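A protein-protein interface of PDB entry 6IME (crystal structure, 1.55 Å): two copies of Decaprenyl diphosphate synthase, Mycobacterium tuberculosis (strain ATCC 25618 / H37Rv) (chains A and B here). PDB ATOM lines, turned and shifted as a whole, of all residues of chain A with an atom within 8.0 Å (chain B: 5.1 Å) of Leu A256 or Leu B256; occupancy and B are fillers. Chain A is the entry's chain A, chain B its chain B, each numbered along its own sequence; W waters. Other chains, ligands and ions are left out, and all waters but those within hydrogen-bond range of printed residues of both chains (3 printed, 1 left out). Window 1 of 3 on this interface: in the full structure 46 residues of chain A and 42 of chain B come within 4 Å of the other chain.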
ATOM      1  N   TYR A 195     -16.933  17.046 -27.207  1.00  0.00           N
ATOM      2  CA  TYR A 195     -15.741  16.354 -27.654  1.00  0.00           C
ATOM      3  C   TYR A 195     -15.298  15.326 -26.619  1.00  0.00           C
ATOM      4  O   TYR A 195     -15.344  15.587 -25.411  1.00  0.00           O
ATOM      5  CB  TYR A 195     -14.613  17.384 -27.913  1.00  0.00           C
ATOM      6  CG  TYR A 195     -13.308  16.714 -28.270  1.00  0.00           C
ATOM      7  CD1 TYR A 195     -12.505  16.136 -27.248  1.00  0.00           C
ATOM      8  CD2 TYR A 195     -12.925  16.540 -29.609  1.00  0.00           C
ATOM      9  CE1 TYR A 195     -11.372  15.431 -27.533  1.00  0.00           C
ATOM     10  CE2 TYR A 195     -11.741  15.837 -29.906  1.00  0.00           C
ATOM     11  CZ  TYR A 195     -11.004  15.268 -28.881  1.00  0.00           C
ATOM     12  OH  TYR A 195      -9.838  14.545 -29.122  1.00  0.00           O
ATOM     13  N   GLY A 196     -14.864  14.152 -27.091  1.00  0.00           N
ATOM     14  CA  GLY A 196     -14.201  13.205 -26.212  1.00  0.00           C
ATOM     15  C   GLY A 196     -13.223  12.404 -27.029  1.00  0.00           C
ATOM     16  O   GLY A 196     -13.586  11.945 -28.112  1.00  0.00           O
ATOM     17  N   GLY A 197     -11.986  12.270 -26.548  1.00  0.00           N
ATOM     18  CA  GLY A 197     -10.935  11.673 -27.362  1.00  0.00           C
ATOM     19  C   GLY A 197     -11.180  10.214 -27.686  1.00  0.00           C
ATOM     20  O   GLY A 197     -11.005   9.789 -28.847  1.00  0.00           O
ATOM     21  N   ARG A 198     -11.624   9.426 -26.690  1.00  0.00           N
ATOM     22  CA  ARG A 198     -11.956   8.037 -26.986  1.00  0.00           C
ATOM     23  C   ARG A 198     -13.091   7.986 -28.002  1.00  0.00           C
ATOM     24  O   ARG A 198     -13.100   7.095 -28.857  1.00  0.00           O
ATOM     25  CB  ARG A 198     -12.390   7.291 -25.720  1.00  0.00           C
ATOM     26  CG  ARG A 198     -11.251   6.963 -24.746  1.00  0.00           C
ATOM     27  CD  ARG A 198     -11.887   6.232 -23.542  1.00  0.00           C
ATOM     28  NE  ARG A 198     -10.831   5.763 -22.612  1.00  0.00           N
ATOM     29  CZ  ARG A 198     -11.101   5.305 -21.400  1.00  0.00           C
ATOM     30  NH1 ARG A 198     -12.375   5.244 -20.970  1.00  0.00           N
ATOM     31  NH2 ARG A 198     -10.118   4.914 -20.599  1.00  0.00           N
ATOM     32  N   THR A 199     -14.090   8.866 -27.850  1.00  0.00           N
ATOM     33  CA  THR A 199     -15.225   8.854 -28.777  1.00  0.00           C
ATOM     34  C   THR A 199     -14.779   9.191 -30.187  1.00  0.00           C
ATOM     35  O   THR A 199     -15.218   8.553 -31.161  1.00  0.00           O
ATOM     36  CB  THR A 199     -16.252   9.878 -28.317  1.00  0.00           C
ATOM     37  OG1 THR A 199     -16.761   9.432 -27.071  1.00  0.00           O
ATOM     38  CG2 THR A 199     -17.413   9.969 -29.301  1.00  0.00           C
ATOM     39  N   GLU A 200     -13.899  10.186 -30.318  1.00  0.00           N
ATOM     40  CA  GLU A 200     -13.330  10.550 -31.623  1.00  0.00           C
ATOM     41  C   GLU A 200     -12.607   9.381 -32.294  1.00  0.00           C
ATOM     42  O   GLU A 200     -12.775   9.134 -33.500  1.00  0.00           O
ATOM     43  CB  GLU A 200     -12.360  11.725 -31.374  1.00  0.00           C
ATOM     44  CG  GLU A 200     -11.630  12.154 -32.563  1.00  0.00           C
ATOM     45  CD  GLU A 200     -10.906  13.428 -32.335  1.00  0.00           C
ATOM     46  OE1 GLU A 200      -9.863  13.461 -31.611  1.00  0.00           O
ATOM     47  OE2 GLU A 200     -11.341  14.420 -32.934  1.00  0.00           O
ATOM     48  N   ILE A 201     -11.799   8.658 -31.532  1.00  0.00           N
ATOM     49  CA  ILE A 201     -11.116   7.483 -32.065  1.00  0.00           C
ATOM     50  C   ILE A 201     -12.137   6.433 -32.460  1.00  0.00           C
ATOM     51  O   ILE A 201     -11.981   5.741 -33.481  1.00  0.00           O
ATOM     52  CB  ILE A 201     -10.130   6.974 -31.004  1.00  0.00           C
ATOM     53  CG1 ILE A 201      -8.963   7.961 -30.902  1.00  0.00           C
ATOM     54  CG2 ILE A 201      -9.623   5.573 -31.352  1.00  0.00           C
ATOM     55  CD1 ILE A 201      -8.179   7.774 -29.598  1.00  0.00           C
ATOM     56  N   LEU A 231      -9.835  10.484 -38.441  1.00  0.00           N
ATOM     57  CA  LEU A 231     -10.380  11.351 -37.412  1.00  0.00           C
ATOM     58  C   LEU A 231     -11.224  12.446 -38.064  1.00  0.00           C
ATOM     59  O   LEU A 231     -11.096  12.744 -39.246  1.00  0.00           O
ATOM     60  CB  LEU A 231      -9.246  11.937 -36.559  1.00  0.00           C
ATOM     61  CG  LEU A 231      -8.447  10.886 -35.802  1.00  0.00           C
ATOM     62  CD1 LEU A 231      -7.183  11.534 -35.246  1.00  0.00           C
ATOM     63  CD2 LEU A 231      -9.306  10.353 -34.672  1.00  0.00           C
ATOM     64  N   VAL A 239      -0.492  17.791 -30.740  1.00  0.00           N
ATOM     65  CA  VAL A 239      -0.424  18.834 -29.720  1.00  0.00           C
ATOM     66  C   VAL A 239       0.988  18.898 -29.166  1.00  0.00           C
ATOM     67  O   VAL A 239       1.538  17.883 -28.739  1.00  0.00           O
ATOM     68  CB  VAL A 239      -1.412  18.554 -28.586  1.00  0.00           C
ATOM     69  CG1 VAL A 239      -1.257  19.586 -27.462  1.00  0.00           C
ATOM     70  CG2 VAL A 239      -2.888  18.527 -29.085  1.00  0.00           C
ATOM     71  N   PHE A 242       0.145  21.135 -23.827  1.00  0.00           N
ATOM     72  CA  PHE A 242      -1.182  20.879 -23.273  1.00  0.00           C
ATOM     73  C   PHE A 242      -1.287  21.644 -21.967  1.00  0.00           C
ATOM     74  O   PHE A 242      -0.519  21.371 -21.023  1.00  0.00           O
ATOM     75  CB  PHE A 242      -1.355  19.367 -23.047  1.00  0.00           C
ATOM     76  CG  PHE A 242      -2.763  18.940 -22.686  1.00  0.00           C
ATOM     77  CD1 PHE A 242      -3.330  19.258 -21.453  1.00  0.00           C
ATOM     78  CD2 PHE A 242      -3.524  18.200 -23.615  1.00  0.00           C
ATOM     79  CE1 PHE A 242      -4.662  18.883 -21.137  1.00  0.00           C
ATOM     80  CE2 PHE A 242      -4.826  17.787 -23.308  1.00  0.00           C
ATOM     81  CZ  PHE A 242      -5.394  18.117 -22.029  1.00  0.00           C
ATOM     82  N   SER A 251      -5.670  15.156 -18.313  1.00  0.00           N
ATOM     83  CA  SER A 251      -6.029  15.585 -19.662  1.00  0.00           C
ATOM     84  C   SER A 251      -7.508  15.421 -19.935  1.00  0.00           C
ATOM     85  O   SER A 251      -8.020  16.080 -20.844  1.00  0.00           O
ATOM     86  CB  SER A 251      -5.235  14.780 -20.708  1.00  0.00           C
ATOM     87  OG  SER A 251      -5.770  13.450 -20.885  1.00  0.00           O
ATOM     88  N   SER A 252      -8.199  14.604 -19.131  1.00  0.00           N
ATOM     89  CA  SER A 252      -9.660  14.420 -19.246  1.00  0.00           C
ATOM     90  C   SER A 252     -10.092  14.200 -20.692  1.00  0.00           C
ATOM     91  O   SER A 252     -11.071  14.804 -21.169  1.00  0.00           O
ATOM     92  CB  SER A 252     -10.421  15.585 -18.629  1.00  0.00           C
ATOM     93  OG  SER A 252     -10.184  15.572 -17.236  1.00  0.00           O
ATOM     94  N   ASN A 253      -9.381  13.301 -21.379  1.00  0.00           N
ATOM     95  CA  ASN A 253      -9.807  12.761 -22.662  1.00  0.00           C
ATOM     96  C   ASN A 253      -9.763  13.838 -23.747  1.00  0.00           C
ATOM     97  O   ASN A 253     -10.384  13.678 -24.797  1.00  0.00           O
ATOM     98  CB  ASN A 253     -11.248  12.194 -22.493  1.00  0.00           C
ATOM     99  CG  ASN A 253     -11.690  11.169 -23.568  1.00  0.00           C
ATOM    100  OD1 ASN A 253     -10.901  10.457 -24.186  1.00  0.00           O
ATOM    101  ND2 ASN A 253     -13.020  11.116 -23.734  1.00  0.00           N
ATOM    102  N   PHE A 254      -9.011  14.921 -23.562  1.00  0.00           N
ATOM    103  CA  PHE A 254      -8.969  15.997 -24.549  1.00  0.00           C
ATOM    104  C   PHE A 254      -7.827  15.774 -25.533  1.00  0.00           C
ATOM    105  O   PHE A 254      -6.694  15.495 -25.125  1.00  0.00           O
ATOM    106  CB  PHE A 254      -8.769  17.351 -23.847  1.00  0.00           C
ATOM    107  CG  PHE A 254      -8.934  18.527 -24.770  1.00  0.00           C
ATOM    108  CD1 PHE A 254     -10.016  18.539 -25.675  1.00  0.00           C
ATOM    109  CD2 PHE A 254      -8.016  19.584 -24.779  1.00  0.00           C
ATOM    110  CE1 PHE A 254     -10.160  19.651 -26.572  1.00  0.00           C
ATOM    111  CE2 PHE A 254      -8.180  20.674 -25.651  1.00  0.00           C
ATOM    112  CZ  PHE A 254      -9.246  20.686 -26.570  1.00  0.00           C
ATOM    113  N   MET A 255      -8.127  15.876 -26.827  1.00  0.00           N
ATOM    114  CA  MET A 255      -7.116  15.663 -27.852  1.00  0.00           C
ATOM    115  C   MET A 255      -6.317  14.386 -27.614  1.00  0.00           C
ATOM    116  O   MET A 255      -5.090  14.363 -27.698  1.00  0.00           O
ATOM    117  CB  MET A 255      -6.161  16.856 -27.983  1.00  0.00           C
ATOM    118  CG  MET A 255      -6.798  18.181 -28.371  1.00  0.00           C
ATOM    119  SD  MET A 255      -8.308  18.285 -29.326  1.00  0.00           S
ATOM    120  CE  MET A 255      -7.341  17.784 -30.738  1.00  0.00           C
ATOM    121  N   LEU A 256      -7.026  13.288 -27.367  1.00  0.00           N
ATOM    122  CA  LEU A 256      -6.380  12.087 -26.830  1.00  0.00           C
ATOM    123  C   LEU A 256      -5.367  11.523 -27.817  1.00  0.00           C
ATOM    124  O   LEU A 256      -4.194  11.308 -27.460  1.00  0.00           O
ATOM    125  CB  LEU A 256      -7.452  11.048 -26.452  1.00  0.00           C
ATOM    126  CG  LEU A 256      -6.863   9.786 -25.831  1.00  0.00           C
ATOM    127  CD1 LEU A 256      -6.198  10.075 -24.503  1.00  0.00           C
ATOM    128  CD2 LEU A 256      -7.973   8.740 -25.651  1.00  0.00           C
ATOM    129  N   TRP A 257      -5.791  11.304 -29.062  1.00  0.00           N
ATOM    130  CA  TRP A 257      -4.841  10.798 -30.057  1.00  0.00           C
ATOM    131  C   TRP A 257      -3.726  11.800 -30.306  1.00  0.00           C
ATOM    132  O   TRP A 257      -2.547  11.426 -30.396  1.00  0.00           O
ATOM    133  CB  TRP A 257      -5.611  10.525 -31.354  1.00  0.00           C
ATOM    134  CG  TRP A 257      -4.734   9.943 -32.455  1.00  0.00           C
ATOM    135  CD1 TRP A 257      -4.036  10.645 -33.424  1.00  0.00           C
ATOM    136  CD2 TRP A 257      -4.484   8.553 -32.716  1.00  0.00           C
ATOM    137  NE1 TRP A 257      -3.372   9.766 -34.257  1.00  0.00           N
ATOM    138  CE2 TRP A 257      -3.624   8.487 -33.842  1.00  0.00           C
ATOM    139  CE3 TRP A 257      -4.922   7.360 -32.121  1.00  0.00           C
ATOM    140  CZ2 TRP A 257      -3.196   7.270 -34.384  1.00  0.00           C
ATOM    141  CZ3 TRP A 257      -4.483   6.147 -32.664  1.00  0.00           C
ATOM    142  CH2 TRP A 257      -3.635   6.125 -33.780  1.00  0.00           C
ATOM    143  N   GLN A 258      -4.104  13.079 -30.460  1.00  0.00           N
ATOM    144  CA  GLN A 258      -3.182  14.114 -30.911  1.00  0.00           C
ATOM    145  C   GLN A 258      -2.152  14.514 -29.856  1.00  0.00           C
ATOM    146  O   GLN A 258      -1.092  15.045 -30.222  1.00  0.00           O
ATOM    147  CB  GLN A 258      -3.949  15.369 -31.309  1.00  0.00           C
ATOM    148  CG  GLN A 258      -5.045  15.106 -32.403  1.00  0.00           C
ATOM    149  CD  GLN A 258      -6.398  14.672 -31.860  1.00  0.00           C
ATOM    150  OE1 GLN A 258      -6.541  14.256 -30.688  1.00  0.00           O
ATOM    151  NE2 GLN A 258      -7.427  14.772 -32.705  1.00  0.00           N
ATOM    152  N   ALA A 259      -2.438  14.306 -28.567  1.00  0.00           N
ATOM    153  CA  ALA A 259      -1.565  14.778 -27.495  1.00  0.00           C
ATOM    154  C   ALA A 259      -0.683  13.663 -26.917  1.00  0.00           C
ATOM    155  O   ALA A 259      -0.046  13.854 -25.879  1.00  0.00           O
ATOM    156  CB  ALA A 259      -2.432  15.412 -26.398  1.00  0.00           C
ATOM    157  N   ALA A 260      -0.555  12.528 -27.610  1.00  0.00           N
ATOM    158  CA  ALA A 260       0.268  11.427 -27.114  1.00  0.00           C
ATOM    159  C   ALA A 260       1.690  11.849 -26.728  1.00  0.00           C
ATOM    160  O   ALA A 260       2.263  11.308 -25.769  1.00  0.00           O
ATOM    161  CB  ALA A 260       0.348  10.328 -28.193  1.00  0.00           C
ATOM    162  N   TYR A 261       2.296  12.814 -27.440  1.00  0.00           N
ATOM    163  CA  TYR A 261       3.635  13.289 -27.088  1.00  0.00           C
ATOM    164  C   TYR A 261       3.656  14.746 -26.626  1.00  0.00           C
ATOM    165  O   TYR A 261       4.714  15.389 -26.594  1.00  0.00           O
ATOM    166  CB  TYR A 261       4.617  13.076 -28.252  1.00  0.00           C
ATOM    167  CG  TYR A 261       5.335  11.723 -28.088  1.00  0.00           C
ATOM    168  CD1 TYR A 261       6.452  11.582 -27.258  1.00  0.00           C
ATOM    169  CD2 TYR A 261       4.833  10.591 -28.699  1.00  0.00           C
ATOM    170  CE1 TYR A 261       7.084  10.321 -27.083  1.00  0.00           C
ATOM    171  CE2 TYR A 261       5.413   9.362 -28.553  1.00  0.00           C
ATOM    172  CZ  TYR A 261       6.532   9.223 -27.725  1.00  0.00           C
ATOM    173  OH  TYR A 261       7.102   7.968 -27.582  1.00  0.00           O
ATOM    174  N   ALA A 262       2.504  15.277 -26.232  1.00  0.00           N
ATOM    175  CA  ALA A 262       2.467  16.660 -25.798  1.00  0.00           C
ATOM    176  C   ALA A 262       3.241  16.846 -24.491  1.00  0.00           C
ATOM    177  O   ALA A 262       3.297  15.957 -23.624  1.00  0.00           O
ATOM    178  CB  ALA A 262       1.003  17.080 -25.576  1.00  0.00           C
ATOM    179  N   TYR A 264       3.027  18.649 -20.934  1.00  0.00           N
ATOM    180  CA  TYR A 264       1.988  19.156 -20.040  1.00  0.00           C
ATOM    181  C   TYR A 264       2.532  20.292 -19.193  1.00  0.00           C
ATOM    182  O   TYR A 264       3.610  20.160 -18.582  1.00  0.00           O
ATOM    183  CB  TYR A 264       1.471  18.030 -19.130  1.00  0.00           C
ATOM    184  CG  TYR A 264       0.635  17.023 -19.850  1.00  0.00           C
ATOM    185  CD1 TYR A 264      -0.696  17.300 -20.122  1.00  0.00           C
ATOM    186  CD2 TYR A 264       1.177  15.826 -20.301  1.00  0.00           C
ATOM    187  CE1 TYR A 264      -1.501  16.404 -20.809  1.00  0.00           C
ATOM    188  CE2 TYR A 264       0.367  14.901 -21.013  1.00  0.00           C
ATOM    189  CZ  TYR A 264      -0.969  15.225 -21.250  1.00  0.00           C
ATOM    190  OH  TYR A 264      -1.856  14.379 -21.951  1.00  0.00           O
ATOM    191  N   TYR B 195       5.724  -1.104 -26.391  1.00  0.00           N
ATOM    192  CA  TYR B 195       4.369  -0.625 -26.188  1.00  0.00           C
ATOM    193  C   TYR B 195       4.237   0.761 -26.805  1.00  0.00           C
ATOM    194  O   TYR B 195       5.103   1.620 -26.617  1.00  0.00           O
ATOM    195  CB  TYR B 195       4.038  -0.605 -24.683  1.00  0.00           C
ATOM    196  CG  TYR B 195       2.663   0.004 -24.465  1.00  0.00           C
ATOM    197  CD1 TYR B 195       2.505   1.390 -24.506  1.00  0.00           C
ATOM    198  CD2 TYR B 195       1.497  -0.813 -24.365  1.00  0.00           C
ATOM    199  CE1 TYR B 195       1.241   1.965 -24.421  1.00  0.00           C
ATOM    200  CE2 TYR B 195       0.201  -0.230 -24.240  1.00  0.00           C
ATOM    201  CZ  TYR B 195       0.098   1.160 -24.295  1.00  0.00           C
ATOM    202  OH  TYR B 195      -1.163   1.747 -24.226  1.00  0.00           O
ATOM    203  N   GLY B 197       0.760   3.570 -27.303  1.00  0.00           N
ATOM    204  CA  GLY B 197      -0.697   3.660 -27.164  1.00  0.00           C
ATOM    205  C   GLY B 197      -1.416   3.780 -28.499  1.00  0.00           C
ATOM    206  O   GLY B 197      -2.451   3.135 -28.713  1.00  0.00           O
ATOM    207  N   ARG B 198      -0.854   4.577 -29.420  1.00  0.00           N
ATOM    208  CA  ARG B 198      -1.463   4.704 -30.753  1.00  0.00           C
ATOM    209  C   ARG B 198      -1.421   3.374 -31.484  1.00  0.00           C
ATOM    210  O   ARG B 198      -2.417   2.991 -32.122  1.00  0.00           O
ATOM    211  CB  ARG B 198      -0.745   5.771 -31.596  1.00  0.00           C
ATOM    212  CG  ARG B 198      -1.080   7.219 -31.171  1.00  0.00           C
ATOM    213  CD  ARG B 198      -0.354   8.151 -32.133  1.00  0.00           C
ATOM    214  NE  ARG B 198      -0.652   9.558 -31.839  1.00  0.00           N
ATOM    215  CZ  ARG B 198       0.011  10.564 -32.412  1.00  0.00           C
ATOM    216  NH1 ARG B 198       0.973  10.294 -33.329  1.00  0.00           N
ATOM    217  NH2 ARG B 198      -0.266  11.839 -32.098  1.00  0.00           N
ATOM    218  N   ILE B 201      -4.104   0.951 -30.077  1.00  0.00           N
ATOM    219  CA  ILE B 201      -5.425   1.278 -30.609  1.00  0.00           C
ATOM    220  C   ILE B 201      -5.544   0.833 -32.064  1.00  0.00           C
ATOM    221  O   ILE B 201      -6.593   0.303 -32.488  1.00  0.00           O
ATOM    222  CB  ILE B 201      -5.658   2.783 -30.441  1.00  0.00           C
ATOM    223  CG1 ILE B 201      -5.892   3.083 -28.950  1.00  0.00           C
ATOM    224  CG2 ILE B 201      -6.928   3.199 -31.185  1.00  0.00           C
ATOM    225  CD1 ILE B 201      -5.717   4.546 -28.615  1.00  0.00           C
ATOM    226  N   ASN B 253       2.914   8.598 -25.002  1.00  0.00           N
ATOM    227  CA  ASN B 253       2.153   7.548 -25.665  1.00  0.00           C
ATOM    228  C   ASN B 253       1.945   6.333 -24.779  1.00  0.00           C
ATOM    229  O   ASN B 253       1.580   5.246 -25.276  1.00  0.00           O
ATOM    230  CB  ASN B 253       2.898   7.189 -26.972  1.00  0.00           C
ATOM    231  CG  ASN B 253       2.050   6.478 -28.022  1.00  0.00           C
ATOM    232  OD1 ASN B 253       0.844   6.597 -28.111  1.00  0.00           O
ATOM    233  ND2 ASN B 253       2.772   5.734 -28.869  1.00  0.00           N
ATOM    234  N   PHE B 254       2.089   6.463 -23.453  1.00  0.00           N
ATOM    235  CA  PHE B 254       1.934   5.307 -22.582  1.00  0.00           C
ATOM    236  C   PHE B 254       0.482   5.194 -22.133  1.00  0.00           C
ATOM    237  O   PHE B 254      -0.122   6.185 -21.676  1.00  0.00           O
ATOM    238  CB  PHE B 254       2.837   5.443 -21.344  1.00  0.00           C
ATOM    239  CG  PHE B 254       2.894   4.194 -20.521  1.00  0.00           C
ATOM    240  CD1 PHE B 254       3.049   2.967 -21.162  1.00  0.00           C
ATOM    241  CD2 PHE B 254       2.812   4.238 -19.109  1.00  0.00           C
ATOM    242  CE1 PHE B 254       3.178   1.775 -20.418  1.00  0.00           C
ATOM    243  CE2 PHE B 254       2.895   3.048 -18.350  1.00  0.00           C
ATOM    244  CZ  PHE B 254       3.062   1.812 -18.993  1.00  0.00           C
ATOM    245  N   MET B 255      -0.062   3.972 -22.185  1.00  0.00           N
ATOM    246  CA  MET B 255      -1.426   3.708 -21.732  1.00  0.00           C
ATOM    247  C   MET B 255      -2.415   4.731 -22.300  1.00  0.00           C
ATOM    248  O   MET B 255      -3.243   5.295 -21.592  1.00  0.00           O
ATOM    249  CB  MET B 255      -1.493   3.700 -20.188  1.00  0.00           C
ATOM    250  CG  MET B 255      -0.848   2.466 -19.505  1.00  0.00           C
ATOM    251  SD  MET B 255      -1.918   1.001 -19.792  1.00  0.00           S
ATOM    252  CE  MET B 255      -0.712  -0.271 -20.246  1.00  0.00           C
ATOM    253  N   LEU B 256      -2.360   4.958 -23.611  1.00  0.00           N
ATOM    254  CA  LEU B 256      -3.051   6.116 -24.169  1.00  0.00           C
ATOM    255  C   LEU B 256      -4.561   6.008 -23.987  1.00  0.00           C
ATOM    256  O   LEU B 256      -5.182   6.944 -23.484  1.00  0.00           O
ATOM    257  CB  LEU B 256      -2.664   6.258 -25.645  1.00  0.00           C
ATOM    258  CG  LEU B 256      -3.287   7.461 -26.361  1.00  0.00           C
ATOM    259  CD1 LEU B 256      -2.844   8.734 -25.786  1.00  0.00           C
ATOM    260  CD2 LEU B 256      -2.826   7.385 -27.827  1.00  0.00           C
ATOM    261  N   TRP B 257      -5.164   4.888 -24.383  1.00  0.00           N
ATOM    262  CA  TRP B 257      -6.600   4.729 -24.176  1.00  0.00           C
ATOM    263  C   TRP B 257      -6.924   4.679 -22.695  1.00  0.00           C
ATOM    264  O   TRP B 257      -7.876   5.316 -22.227  1.00  0.00           O
ATOM    265  CB  TRP B 257      -7.058   3.432 -24.850  1.00  0.00           C
ATOM    266  CG  TRP B 257      -8.511   3.188 -24.743  1.00  0.00           C
ATOM    267  CD1 TRP B 257      -9.195   2.507 -23.745  1.00  0.00           C
ATOM    268  CD2 TRP B 257      -9.490   3.552 -25.727  1.00  0.00           C
ATOM    269  NE1 TRP B 257     -10.547   2.488 -24.047  1.00  0.00           N
ATOM    270  CE2 TRP B 257     -10.750   3.117 -25.248  1.00  0.00           C
ATOM    271  CE3 TRP B 257      -9.423   4.276 -26.922  1.00  0.00           C
ATOM    272  CZ2 TRP B 257     -11.954   3.324 -25.964  1.00  0.00           C
ATOM    273  CZ3 TRP B 257     -10.616   4.472 -27.651  1.00  0.00           C
ATOM    274  CH2 TRP B 257     -11.858   4.014 -27.153  1.00  0.00           C
ATOM    275  N   GLN B 258      -6.126   3.909 -21.946  1.00  0.00           N
ATOM    276  CA  GLN B 258      -6.479   3.591 -20.561  1.00  0.00           C
ATOM    277  C   GLN B 258      -6.312   4.755 -19.595  1.00  0.00           C
ATOM    278  O   GLN B 258      -7.013   4.790 -18.570  1.00  0.00           O
ATOM    279  CB  GLN B 258      -5.601   2.425 -20.059  1.00  0.00           C
ATOM    280  CG  GLN B 258      -5.704   1.113 -20.877  1.00  0.00           C
ATOM    281  CD  GLN B 258      -4.754   1.058 -22.083  1.00  0.00           C
ATOM    282  OE1 GLN B 258      -4.175   2.071 -22.525  1.00  0.00           O
ATOM    283  NE2 GLN B 258      -4.514  -0.174 -22.581  1.00  0.00           N
ATOM    284  N   ALA B 259      -5.436   5.721 -19.904  1.00  0.00           N
ATOM    285  CA  ALA B 259      -5.147   6.851 -19.030  1.00  0.00           C
ATOM    286  C   ALA B 259      -5.854   8.124 -19.454  1.00  0.00           C
ATOM    287  O   ALA B 259      -5.553   9.187 -18.923  1.00  0.00           O
ATOM    288  CB  ALA B 259      -3.624   7.064 -18.955  1.00  0.00           C
ATOM    289  N   ALA B 260      -6.885   8.007 -20.302  1.00  0.00           N
ATOM    290  CA  ALA B 260      -7.607   9.198 -20.760  1.00  0.00           C
ATOM    291  C   ALA B 260      -8.098  10.074 -19.626  1.00  0.00           C
ATOM    292  O   ALA B 260      -8.105  11.309 -19.747  1.00  0.00           O
ATOM    293  CB  ALA B 260      -8.804   8.779 -21.635  1.00  0.00           C
HETATM  294  O   HOH W   1      -6.308  12.556 -17.810  1.00  0.00           O
HETATM  295  O   HOH W   2      -4.196  11.215 -20.598  1.00  0.00           O
HETATM  296  O   HOH W   3      -0.941  10.175 -36.085  1.00  0.00           O
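O of Trp B257 is in hydrogen-bond range of NH2 of Arg A198 (2.8 Å). O of Ala B260 lies within hydrogen-bond range of OG of Ser A251. The backbone carbonyl oxygen (O) of Ala B260 is in hydrogen-bond range of the backbone NH (N) of Ser A252 (3.4 Å). The backbone carbonyl oxygen (O) of Ala B260 is in hydrogen-bond range of the backbone NH (N) of Asn A253. O of Trp A257 sits at hydrogen-bond distance from NH2 of Arg B198. The backbone carbonyl oxygen of Ala A260 is in hydrogen-bond range of the backbone NH of Asn B253 (2.9 Å).
N of Gly A197 sits at hydrogen-bond distance from O of Asn A253 (2.8 Å). The side-chain carboxylate (OE1) of Glu A200 is in hydrogen-bond range of the side-chain amide nitrogen (NE2) of Gln A258 (3.0 Å). O of Gln A258 sits at hydrogen-bond distance from N of Val A239. OH of Tyr B195 sits at hydrogen-bond distance from OE1 of Gln B258, 3.5 Å away. The backbone NH (N) of Arg B198 lies within hydrogen-bond range of the side-chain amide oxygen (OD1) of Asn B253, 2.9 Å away. The side-chain amide oxygen (OE1) of Gln B258 sits close to the backbone carbonyl oxygen (O) of Met B255 (3.5 Å).
Among the printed residues, pairs that only touch across the chains: Arg A198 with Gln B258, Arg A198 with Ala B260, Ile A201 with Ile B201, Ile A201 with Trp B257, Leu A256 with Leu B256, Gln A258 with Arg B198, Ala A260 with Arg B198 and Tyr A261 with Asn B253.
Of the printed residues of chain B, Ile A201 touches Ile B201 and Trp B257. Leu A256 touches just one residue of chain B: Leu B256. Of the printed residues of chain B, Gln A258 touches Arg B198 (3.8 Å). Printed residues of chain B within 4 Å of Ala A260: Arg B198 (3.9 Å) and Asn B253 (2.9 Å). Of the printed residues of chain B, Tyr A261 touches Asn B253. Of chain A, only Leu A256 (3.4 Å) comes within 4 Å of Leu B256. The nearest residue of chain B that does not touch Leu A256 is Ala B260 (4.1 Å). The nearest residue of chain A that does not touch Leu B256 is Ala A260 (4.3 Å).
Among the printed residues, 14 pairs touch across the chains. Among the printed residues, no Asp or Glu carboxylate lies within 4 Å of a Lys or Arg side-chain nitrogen of the other chain.
Arg A198 touches Trp B257, and with the chains exchanged Trp A257 touches Arg B198. Arg A198 touches Gln B258, and with the chains exchanged Gln A258 touches Arg B198. Arg A198 touches Ala B260, and with the chains exchanged Ala A260 touches Arg B198. Ile B201 touches its own counterpart, Ile A201. Of the 14 pairs that touch across the chains among the printed residues, 10 have their exchanged pair printed and touching as well.
Water W1 lies within hydrogen-bond range of the backbone NH (N) of Ser A251 (2.7 Å), the backbone carbonyl oxygen (O) of Ala B260 (2.9 Å) and the backbone NH (N) of Ser A252 (3.1 Å). Water W2 bridges OG of Ser A251 and O of Ala B259. Water W3 lies within hydrogen-bond range of the indole nitrogen (NE1) of Trp A257 (3.1 Å) and the guanidinium group (NH1) of Arg B198 (3.4 Å).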
